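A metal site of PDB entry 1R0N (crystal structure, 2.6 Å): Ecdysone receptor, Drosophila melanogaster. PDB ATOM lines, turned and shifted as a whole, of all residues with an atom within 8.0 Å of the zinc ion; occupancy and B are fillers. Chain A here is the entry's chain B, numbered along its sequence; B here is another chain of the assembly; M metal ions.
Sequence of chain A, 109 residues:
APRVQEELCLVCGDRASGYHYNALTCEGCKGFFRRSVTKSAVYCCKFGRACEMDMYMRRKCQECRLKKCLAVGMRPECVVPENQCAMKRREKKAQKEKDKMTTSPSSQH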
ATOM      1  N   LEU A   8     -36.190 -20.442  12.024  1.00  0.00           N
ATOM      2  CA  LEU A   8     -34.761 -20.091  12.221  1.00  0.00           C
ATOM      3  C   LEU A   8     -34.218 -20.147  13.659  1.00  0.00           C
ATOM      4  O   LEU A   8     -34.850 -19.619  14.564  1.00  0.00           O
ATOM      5  CB  LEU A   8     -34.478 -18.705  11.646  1.00  0.00           C
ATOM      6  CG  LEU A   8     -33.876 -18.602  10.244  1.00  0.00           C
ATOM      7  CD1 LEU A   8     -34.346 -19.739   9.373  1.00  0.00           C
ATOM      8  CD2 LEU A   8     -34.214 -17.231   9.644  1.00  0.00           C
ATOM      9  N   CYS A   9     -33.073 -20.790  13.863  1.00  0.00           N
ATOM     10  CA  CYS A   9     -32.464 -20.846  15.209  1.00  0.00           C
ATOM     11  C   CYS A   9     -32.042 -19.428  15.648  1.00  0.00           C
ATOM     12  O   CYS A   9     -31.250 -18.763  14.991  1.00  0.00           O
ATOM     13  CB  CYS A   9     -31.237 -21.762  15.195  1.00  0.00           C
ATOM     14  SG  CYS A   9     -30.298 -21.760  16.764  1.00  0.00           S
ATOM     15  N   LEU A  10     -32.577 -18.945  16.752  1.00  0.00           N
ATOM     16  CA  LEU A  10     -32.245 -17.584  17.203  1.00  0.00           C
ATOM     17  C   LEU A  10     -30.785 -17.483  17.607  1.00  0.00           C
ATOM     18  O   LEU A  10     -30.282 -16.375  17.783  1.00  0.00           O
ATOM     19  CB  LEU A  10     -33.150 -17.159  18.379  1.00  0.00           C
ATOM     20  CG  LEU A  10     -34.624 -17.130  18.025  1.00  0.00           C
ATOM     21  CD1 LEU A  10     -35.435 -17.410  19.239  1.00  0.00           C
ATOM     22  CD2 LEU A  10     -34.984 -15.799  17.382  1.00  0.00           C
ATOM     23  N   VAL A  11     -30.086 -18.612  17.769  1.00  0.00           N
ATOM     24  CA  VAL A  11     -28.703 -18.461  18.134  1.00  0.00           C
ATOM     25  C   VAL A  11     -27.817 -18.188  16.931  1.00  0.00           C
ATOM     26  O   VAL A  11     -27.274 -17.059  16.788  1.00  0.00           O
ATOM     27  CB  VAL A  11     -28.150 -19.655  18.953  1.00  0.00           C
ATOM     28  CG1 VAL A  11     -26.644 -19.595  19.003  1.00  0.00           C
ATOM     29  CG2 VAL A  11     -28.673 -19.583  20.397  1.00  0.00           C
ATOM     30  N   CYS A  12     -27.718 -19.172  16.049  1.00  0.00           N
ATOM     31  CA  CYS A  12     -26.860 -19.093  14.893  1.00  0.00           C
ATOM     32  C   CYS A  12     -27.532 -18.852  13.553  1.00  0.00           C
ATOM     33  O   CYS A  12     -26.862 -18.614  12.544  1.00  0.00           O
ATOM     34  CB  CYS A  12     -26.034 -20.379  14.802  1.00  0.00           C
ATOM     35  SG  CYS A  12     -27.027 -21.871  14.392  1.00  0.00           S
ATOM     36  N   GLY A  13     -28.851 -18.931  13.493  1.00  0.00           N
ATOM     37  CA  GLY A  13     -29.492 -18.688  12.211  1.00  0.00           C
ATOM     38  C   GLY A  13     -29.608 -19.926  11.368  1.00  0.00           C
ATOM     39  O   GLY A  13     -29.979 -19.868  10.194  1.00  0.00           O
ATOM     40  N   ASP A  14     -29.263 -21.064  11.953  1.00  0.00           N
ATOM     41  CA  ASP A  14     -29.370 -22.324  11.253  1.00  0.00           C
ATOM     42  C   ASP A  14     -30.833 -22.642  11.295  1.00  0.00           C
ATOM     43  O   ASP A  14     -31.616 -21.864  11.847  1.00  0.00           O
ATOM     44  CB  ASP A  14     -28.607 -23.383  12.002  1.00  0.00           C
ATOM     45  CG  ASP A  14     -28.324 -24.607  11.152  1.00  0.00           C
ATOM     46  OD1 ASP A  14     -27.436 -25.358  11.589  1.00  0.00           O
ATOM     47  OD2 ASP A  14     -28.988 -24.816  10.085  1.00  0.00           O
ATOM     48  N   ARG A  15     -31.205 -23.788  10.724  1.00  0.00           N
ATOM     49  CA  ARG A  15     -32.599 -24.212  10.700  1.00  0.00           C
ATOM     50  C   ARG A  15     -33.045 -24.679  12.084  1.00  0.00           C
ATOM     51  O   ARG A  15     -32.467 -25.590  12.649  1.00  0.00           O
ATOM     52  CB  ARG A  15     -32.743 -25.347   9.694  1.00  0.00           C
ATOM     53  CG  ARG A  15     -34.081 -26.095   9.713  1.00  0.00           C
ATOM     54  CD  ARG A  15     -33.879 -27.557   9.257  1.00  0.00           C
ATOM     55  NE  ARG A  15     -35.131 -28.247   8.959  1.00  0.00           N
ATOM     56  CZ  ARG A  15     -35.888 -28.009   7.880  1.00  0.00           C
ATOM     57  NH1 ARG A  15     -35.528 -27.085   6.988  1.00  0.00           N
ATOM     58  NH2 ARG A  15     -37.029 -28.687   7.691  1.00  0.00           N
ATOM     59  N   ALA A  16     -34.067 -24.052  12.651  1.00  0.00           N
ATOM     60  CA  ALA A  16     -34.525 -24.454  13.974  1.00  0.00           C
ATOM     61  C   ALA A  16     -35.339 -25.758  13.991  1.00  0.00           C
ATOM     62  O   ALA A  16     -36.206 -25.982  13.155  1.00  0.00           O
ATOM     63  CB  ALA A  16     -35.340 -23.334  14.581  1.00  0.00           C
ATOM     64  N   LEU A  24     -36.542 -20.783  20.396  1.00  0.00           N
ATOM     65  CA  LEU A  24     -36.457 -21.393  19.074  1.00  0.00           C
ATOM     66  C   LEU A  24     -35.006 -21.511  18.594  1.00  0.00           C
ATOM     67  O   LEU A  24     -34.358 -20.500  18.283  1.00  0.00           O
ATOM     68  CB  LEU A  24     -37.238 -20.544  18.079  1.00  0.00           C
ATOM     69  CG  LEU A  24     -37.486 -21.177  16.722  1.00  0.00           C
ATOM     70  CD1 LEU A  24     -38.081 -22.600  16.860  1.00  0.00           C
ATOM     71  CD2 LEU A  24     -38.434 -20.268  15.943  1.00  0.00           C
ATOM     72  N   THR A  25     -34.524 -22.758  18.526  1.00  0.00           N
ATOM     73  CA  THR A  25     -33.137 -23.049  18.142  1.00  0.00           C
ATOM     74  C   THR A  25     -32.946 -24.258  17.255  1.00  0.00           C
ATOM     75  O   THR A  25     -33.889 -24.954  16.889  1.00  0.00           O
ATOM     76  CB  THR A  25     -32.273 -23.276  19.362  1.00  0.00           C
ATOM     77  OG1 THR A  25     -32.698 -24.467  20.032  1.00  0.00           O
ATOM     78  CG2 THR A  25     -32.408 -22.092  20.303  1.00  0.00           C
ATOM     79  N   CYS A  26     -31.676 -24.516  16.944  1.00  0.00           N
ATOM     80  CA  CYS A  26     -31.261 -25.578  16.075  1.00  0.00           C
ATOM     81  C   CYS A  26     -30.769 -26.709  16.964  1.00  0.00           C
ATOM     82  O   CYS A  26     -30.588 -26.503  18.151  1.00  0.00           O
ATOM     83  CB  CYS A  26     -30.160 -25.083  15.139  1.00  0.00           C
ATOM     84  SG  CYS A  26     -28.523 -25.125  15.797  1.00  0.00           S
ATOM     85  N   GLU A  27     -30.545 -27.897  16.393  1.00  0.00           N
ATOM     86  CA  GLU A  27     -30.092 -29.018  17.187  1.00  0.00           C
ATOM     87  C   GLU A  27     -28.743 -28.837  17.910  1.00  0.00           C
ATOM     88  O   GLU A  27     -28.586 -29.214  19.066  1.00  0.00           O
ATOM     89  CB  GLU A  27     -30.072 -30.296  16.317  1.00  0.00           C
ATOM     90  CG  GLU A  27     -31.447 -30.982  16.194  1.00  0.00           C
ATOM     91  CD  GLU A  27     -32.086 -31.375  17.555  1.00  0.00           C
ATOM     92  OE1 GLU A  27     -31.437 -32.114  18.338  1.00  0.00           O
ATOM     93  OE2 GLU A  27     -33.240 -30.957  17.818  1.00  0.00           O
ATOM     94  N   GLY A  28     -27.758 -28.261  17.261  1.00  0.00           N
ATOM     95  CA  GLY A  28     -26.497 -28.102  17.932  1.00  0.00           C
ATOM     96  C   GLY A  28     -26.529 -27.113  19.071  1.00  0.00           C
ATOM     97  O   GLY A  28     -25.906 -27.337  20.102  1.00  0.00           O
ATOM     98  N   CYS A  29     -27.235 -26.005  18.904  1.00  0.00           N
ATOM     99  CA  CYS A  29     -27.310 -25.032  19.961  1.00  0.00           C
ATOM    100  C   CYS A  29     -28.067 -25.663  21.123  1.00  0.00           C
ATOM    101  O   CYS A  29     -27.738 -25.482  22.307  1.00  0.00           O
ATOM    102  CB  CYS A  29     -27.970 -23.755  19.428  1.00  0.00           C
ATOM    103  SG  CYS A  29     -26.913 -22.821  18.235  1.00  0.00           S
ATOM    104  N   LYS A  30     -29.071 -26.435  20.800  1.00  0.00           N
ATOM    105  CA  LYS A  30     -29.810 -27.115  21.842  1.00  0.00           C
ATOM    106  C   LYS A  30     -28.841 -27.960  22.682  1.00  0.00           C
ATOM    107  O   LYS A  30     -28.702 -27.732  23.887  1.00  0.00           O
ATOM    108  CB  LYS A  30     -30.869 -28.018  21.201  1.00  0.00           C
ATOM    109  CG  LYS A  30     -31.239 -29.209  22.054  1.00  0.00           C
ATOM    110  CD  LYS A  30     -32.025 -30.207  21.235  1.00  0.00           C
ATOM    111  CE  LYS A  30     -32.193 -31.502  21.968  1.00  0.00           C
ATOM    112  NZ  LYS A  30     -33.033 -32.413  21.161  1.00  0.00           N
ATOM    113  N   MET A  53     -22.640 -14.491  15.817  1.00  0.00           N
ATOM    114  CA  MET A  53     -22.869 -15.897  15.542  1.00  0.00           C
ATOM    115  C   MET A  53     -23.518 -16.277  14.224  1.00  0.00           C
ATOM    116  O   MET A  53     -24.456 -15.671  13.759  1.00  0.00           O
ATOM    117  CB  MET A  53     -23.688 -16.486  16.691  1.00  0.00           C
ATOM    118  CG  MET A  53     -23.003 -16.385  18.041  1.00  0.00           C
ATOM    119  SD  MET A  53     -21.618 -17.528  18.158  1.00  0.00           S
ATOM    120  CE  MET A  53     -22.442 -18.834  18.679  1.00  0.00           C
ATOM    121  N   ASP A  54     -22.966 -17.301  13.630  1.00  0.00           N
ATOM    122  CA  ASP A  54     -23.489 -17.837  12.388  1.00  0.00           C
ATOM    123  C   ASP A  54     -23.113 -19.291  12.436  1.00  0.00           C
ATOM    124  O   ASP A  54     -22.580 -19.746  13.428  1.00  0.00           O
ATOM    125  CB  ASP A  54     -22.885 -17.128  11.150  1.00  0.00           C
ATOM    126  CG  ASP A  54     -21.351 -17.170  11.081  1.00  0.00           C
ATOM    127  OD1 ASP A  54     -20.731 -18.045  11.735  1.00  0.00           O
ATOM    128  OD2 ASP A  54     -20.784 -16.324  10.338  1.00  0.00           O
ATOM    129  N   MET A  55     -23.377 -20.013  11.358  1.00  0.00           N
ATOM    130  CA  MET A  55     -23.075 -21.455  11.298  1.00  0.00           C
ATOM    131  C   MET A  55     -21.618 -21.801  11.465  1.00  0.00           C
ATOM    132  O   MET A  55     -21.301 -22.829  12.009  1.00  0.00           O
ATOM    133  CB  MET A  55     -23.627 -22.035  10.025  1.00  0.00           C
ATOM    134  CG  MET A  55     -25.168 -22.100  10.058  1.00  0.00           C
ATOM    135  SD  MET A  55     -25.814 -23.337   8.867  1.00  0.00           S
ATOM    136  CE  MET A  55     -25.227 -24.861   9.602  1.00  0.00           C
ATOM    137  N   ARG A  58     -20.272 -20.179  15.448  1.00  0.00           N
ATOM    138  CA  ARG A  58     -20.820 -20.803  16.626  1.00  0.00           C
ATOM    139  C   ARG A  58     -19.858 -21.849  17.178  1.00  0.00           C
ATOM    140  O   ARG A  58     -19.660 -21.949  18.381  1.00  0.00           O
ATOM    141  CB  ARG A  58     -22.223 -21.401  16.324  1.00  0.00           C
ATOM    142  CG  ARG A  58     -22.286 -22.819  15.653  1.00  0.00           C
ATOM    143  CD  ARG A  58     -23.696 -23.180  15.154  1.00  0.00           C
ATOM    144  NE  ARG A  58     -23.668 -24.539  14.636  1.00  0.00           N
ATOM    145  CZ  ARG A  58     -24.610 -25.172  13.943  1.00  0.00           C
ATOM    146  NH1 ARG A  58     -25.784 -24.605  13.621  1.00  0.00           N
ATOM    147  NH2 ARG A  58     -24.367 -26.405  13.548  1.00  0.00           N
ATOM    148  N   ARG A  65     -21.196 -18.256  22.212  1.00  0.00           N
ATOM    149  CA  ARG A  65     -22.365 -19.025  21.833  1.00  0.00           C
ATOM    150  C   ARG A  65     -23.284 -19.111  23.046  1.00  0.00           C
ATOM    151  O   ARG A  65     -24.504 -19.002  22.920  1.00  0.00           O
ATOM    152  CB  ARG A  65     -21.961 -20.409  21.375  1.00  0.00           C
ATOM    153  CG  ARG A  65     -23.104 -21.216  20.823  1.00  0.00           C
ATOM    154  CD  ARG A  65     -22.572 -22.478  20.280  1.00  0.00           C
ATOM    155  NE  ARG A  65     -23.567 -23.293  19.568  1.00  0.00           N
ATOM    156  CZ  ARG A  65     -23.275 -24.453  19.001  1.00  0.00           C
ATOM    157  NH1 ARG A  65     -22.038 -24.929  19.078  1.00  0.00           N
ATOM    158  NH2 ARG A  65     -24.190 -25.117  18.313  1.00  0.00           N
ATOM    159  N   CYS A  69     -27.121 -17.933  23.728  1.00  0.00           N
ATOM    160  CA  CYS A  69     -28.162 -18.904  24.019  1.00  0.00           C
ATOM    161  C   CYS A  69     -29.001 -18.259  25.093  1.00  0.00           C
ATOM    162  O   CYS A  69     -30.222 -18.196  25.027  1.00  0.00           O
ATOM    163  CB  CYS A  69     -27.575 -20.217  24.568  1.00  0.00           C
ATOM    164  SG  CYS A  69     -26.793 -21.296  23.318  1.00  0.00           S
ATOM    165  N   MET A  74     -33.154 -18.804  26.291  1.00  0.00           N
ATOM    166  CA  MET A  74     -32.954 -20.210  26.608  1.00  0.00           C
ATOM    167  C   MET A  74     -32.661 -20.315  28.102  1.00  0.00           C
ATOM    168  O   MET A  74     -31.621 -19.844  28.548  1.00  0.00           O
ATOM    169  CB  MET A  74     -31.758 -20.672  25.805  1.00  0.00           C
ATOM    170  CG  MET A  74     -31.893 -21.993  25.112  1.00  0.00           C
ATOM    171  SD  MET A  74     -30.606 -21.982  23.922  1.00  0.00           S
ATOM    172  CE  MET A  74     -30.591 -23.778  23.468  1.00  0.00           C
ATOM    173  P    DG B  12     -22.187 -27.726  16.295  1.00  0.00           P
ATOM    174  OP1  DG B  12     -21.943 -26.860  15.105  1.00  0.00           O
ATOM    175  OP2  DG B  12     -22.796 -27.169  17.521  1.00  0.00           O
ATOM    176  O5'  DG B  12     -23.079 -28.955  15.846  1.00  0.00           O
ATOM    177  C5'  DG B  12     -22.752 -29.648  14.641  1.00  0.00           C
ATOM    178  C4'  DG B  12     -23.618 -30.875  14.502  1.00  0.00           C
ATOM    179  O4'  DG B  12     -23.298 -31.761  15.598  1.00  0.00           O
ATOM    180  C3'  DG B  12     -25.126 -30.637  14.570  1.00  0.00           C
ATOM    181  O3'  DG B  12     -25.765 -31.563  13.718  1.00  0.00           O
ATOM    182  C2'  DG B  12     -25.473 -31.050  15.981  1.00  0.00           C
ATOM    183  C1'  DG B  12     -24.508 -32.201  16.167  1.00  0.00           C
ATOM    184  N9   DG B  12     -24.252 -32.612  17.549  1.00  0.00           N
ATOM    185  C8   DG B  12     -24.152 -31.820  18.650  1.00  0.00           C
ATOM    186  N7   DG B  12     -23.930 -32.502  19.747  1.00  0.00           N
ATOM    187  C5   DG B  12     -23.892 -33.813  19.330  1.00  0.00           C
ATOM    188  C6   DG B  12     -23.668 -34.998  20.059  1.00  0.00           C
ATOM    189  O6   DG B  12     -23.499 -35.143  21.286  1.00  0.00           O
ATOM    190  N1   DG B  12     -23.648 -36.112  19.238  1.00  0.00           N
ATOM    191  C2   DG B  12     -23.848 -36.085  17.889  1.00  0.00           C
ATOM    192  N2   DG B  12     -23.842 -37.266  17.266  1.00  0.00           N
ATOM    193  N3   DG B  12     -24.060 -34.990  17.201  1.00  0.00           N
ATOM    194  C4   DG B  12     -24.063 -33.900  17.977  1.00  0.00           C
HETATM  195 ZN    ZN M   1     -28.240 -22.429  16.458  1.00  0.00          ZN
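The side-chain sulfur of Cys 9 lies close to the backbone NH of Val 11.
The backbone carbonyl oxygen of Asp 14 is in hydrogen-bond range of the backbone NH of Cys 9 (2.7 Å).
The side-chain sulfur (SG) of Cys 29 sits close to the guanidinium group (NH2) of Arg 65 (3.6 Å).
NH1 of Arg 58 sits close to SG of Cys 12 of chain A (3.1 Å).
The backbone NH (N) of Asp 14 sits close to the side-chain sulfur (SG) of Cys 12 of chain A, 3.4 Å away.
SG of Cys 26 sits close to NH1 of Arg 58 (3.5 Å).
The backbone NH (N) of Gly 28 lies close to the side-chain sulfur (SG) of Cys 26.
Merely in contact with the zinc ion: Val 11 (3.7 Å).
Of the 24 residues printed, 5 come within 4 Å of the zinc ion.
The nearest printed residue that does not touch the zinc ion is Arg 58 (4.3 Å).
SG of Cys 9 binds the zinc ion.
The zinc ion is bound by the side-chain sulfur (SG) of Cys 29, at 2.3 Å.
The zinc ion is bound by the side-chain sulfur (SG) of Cys 12 of chain A (2.5 Å).
The zinc ion is bound by SG of Cys 26, at 2.8 Å.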
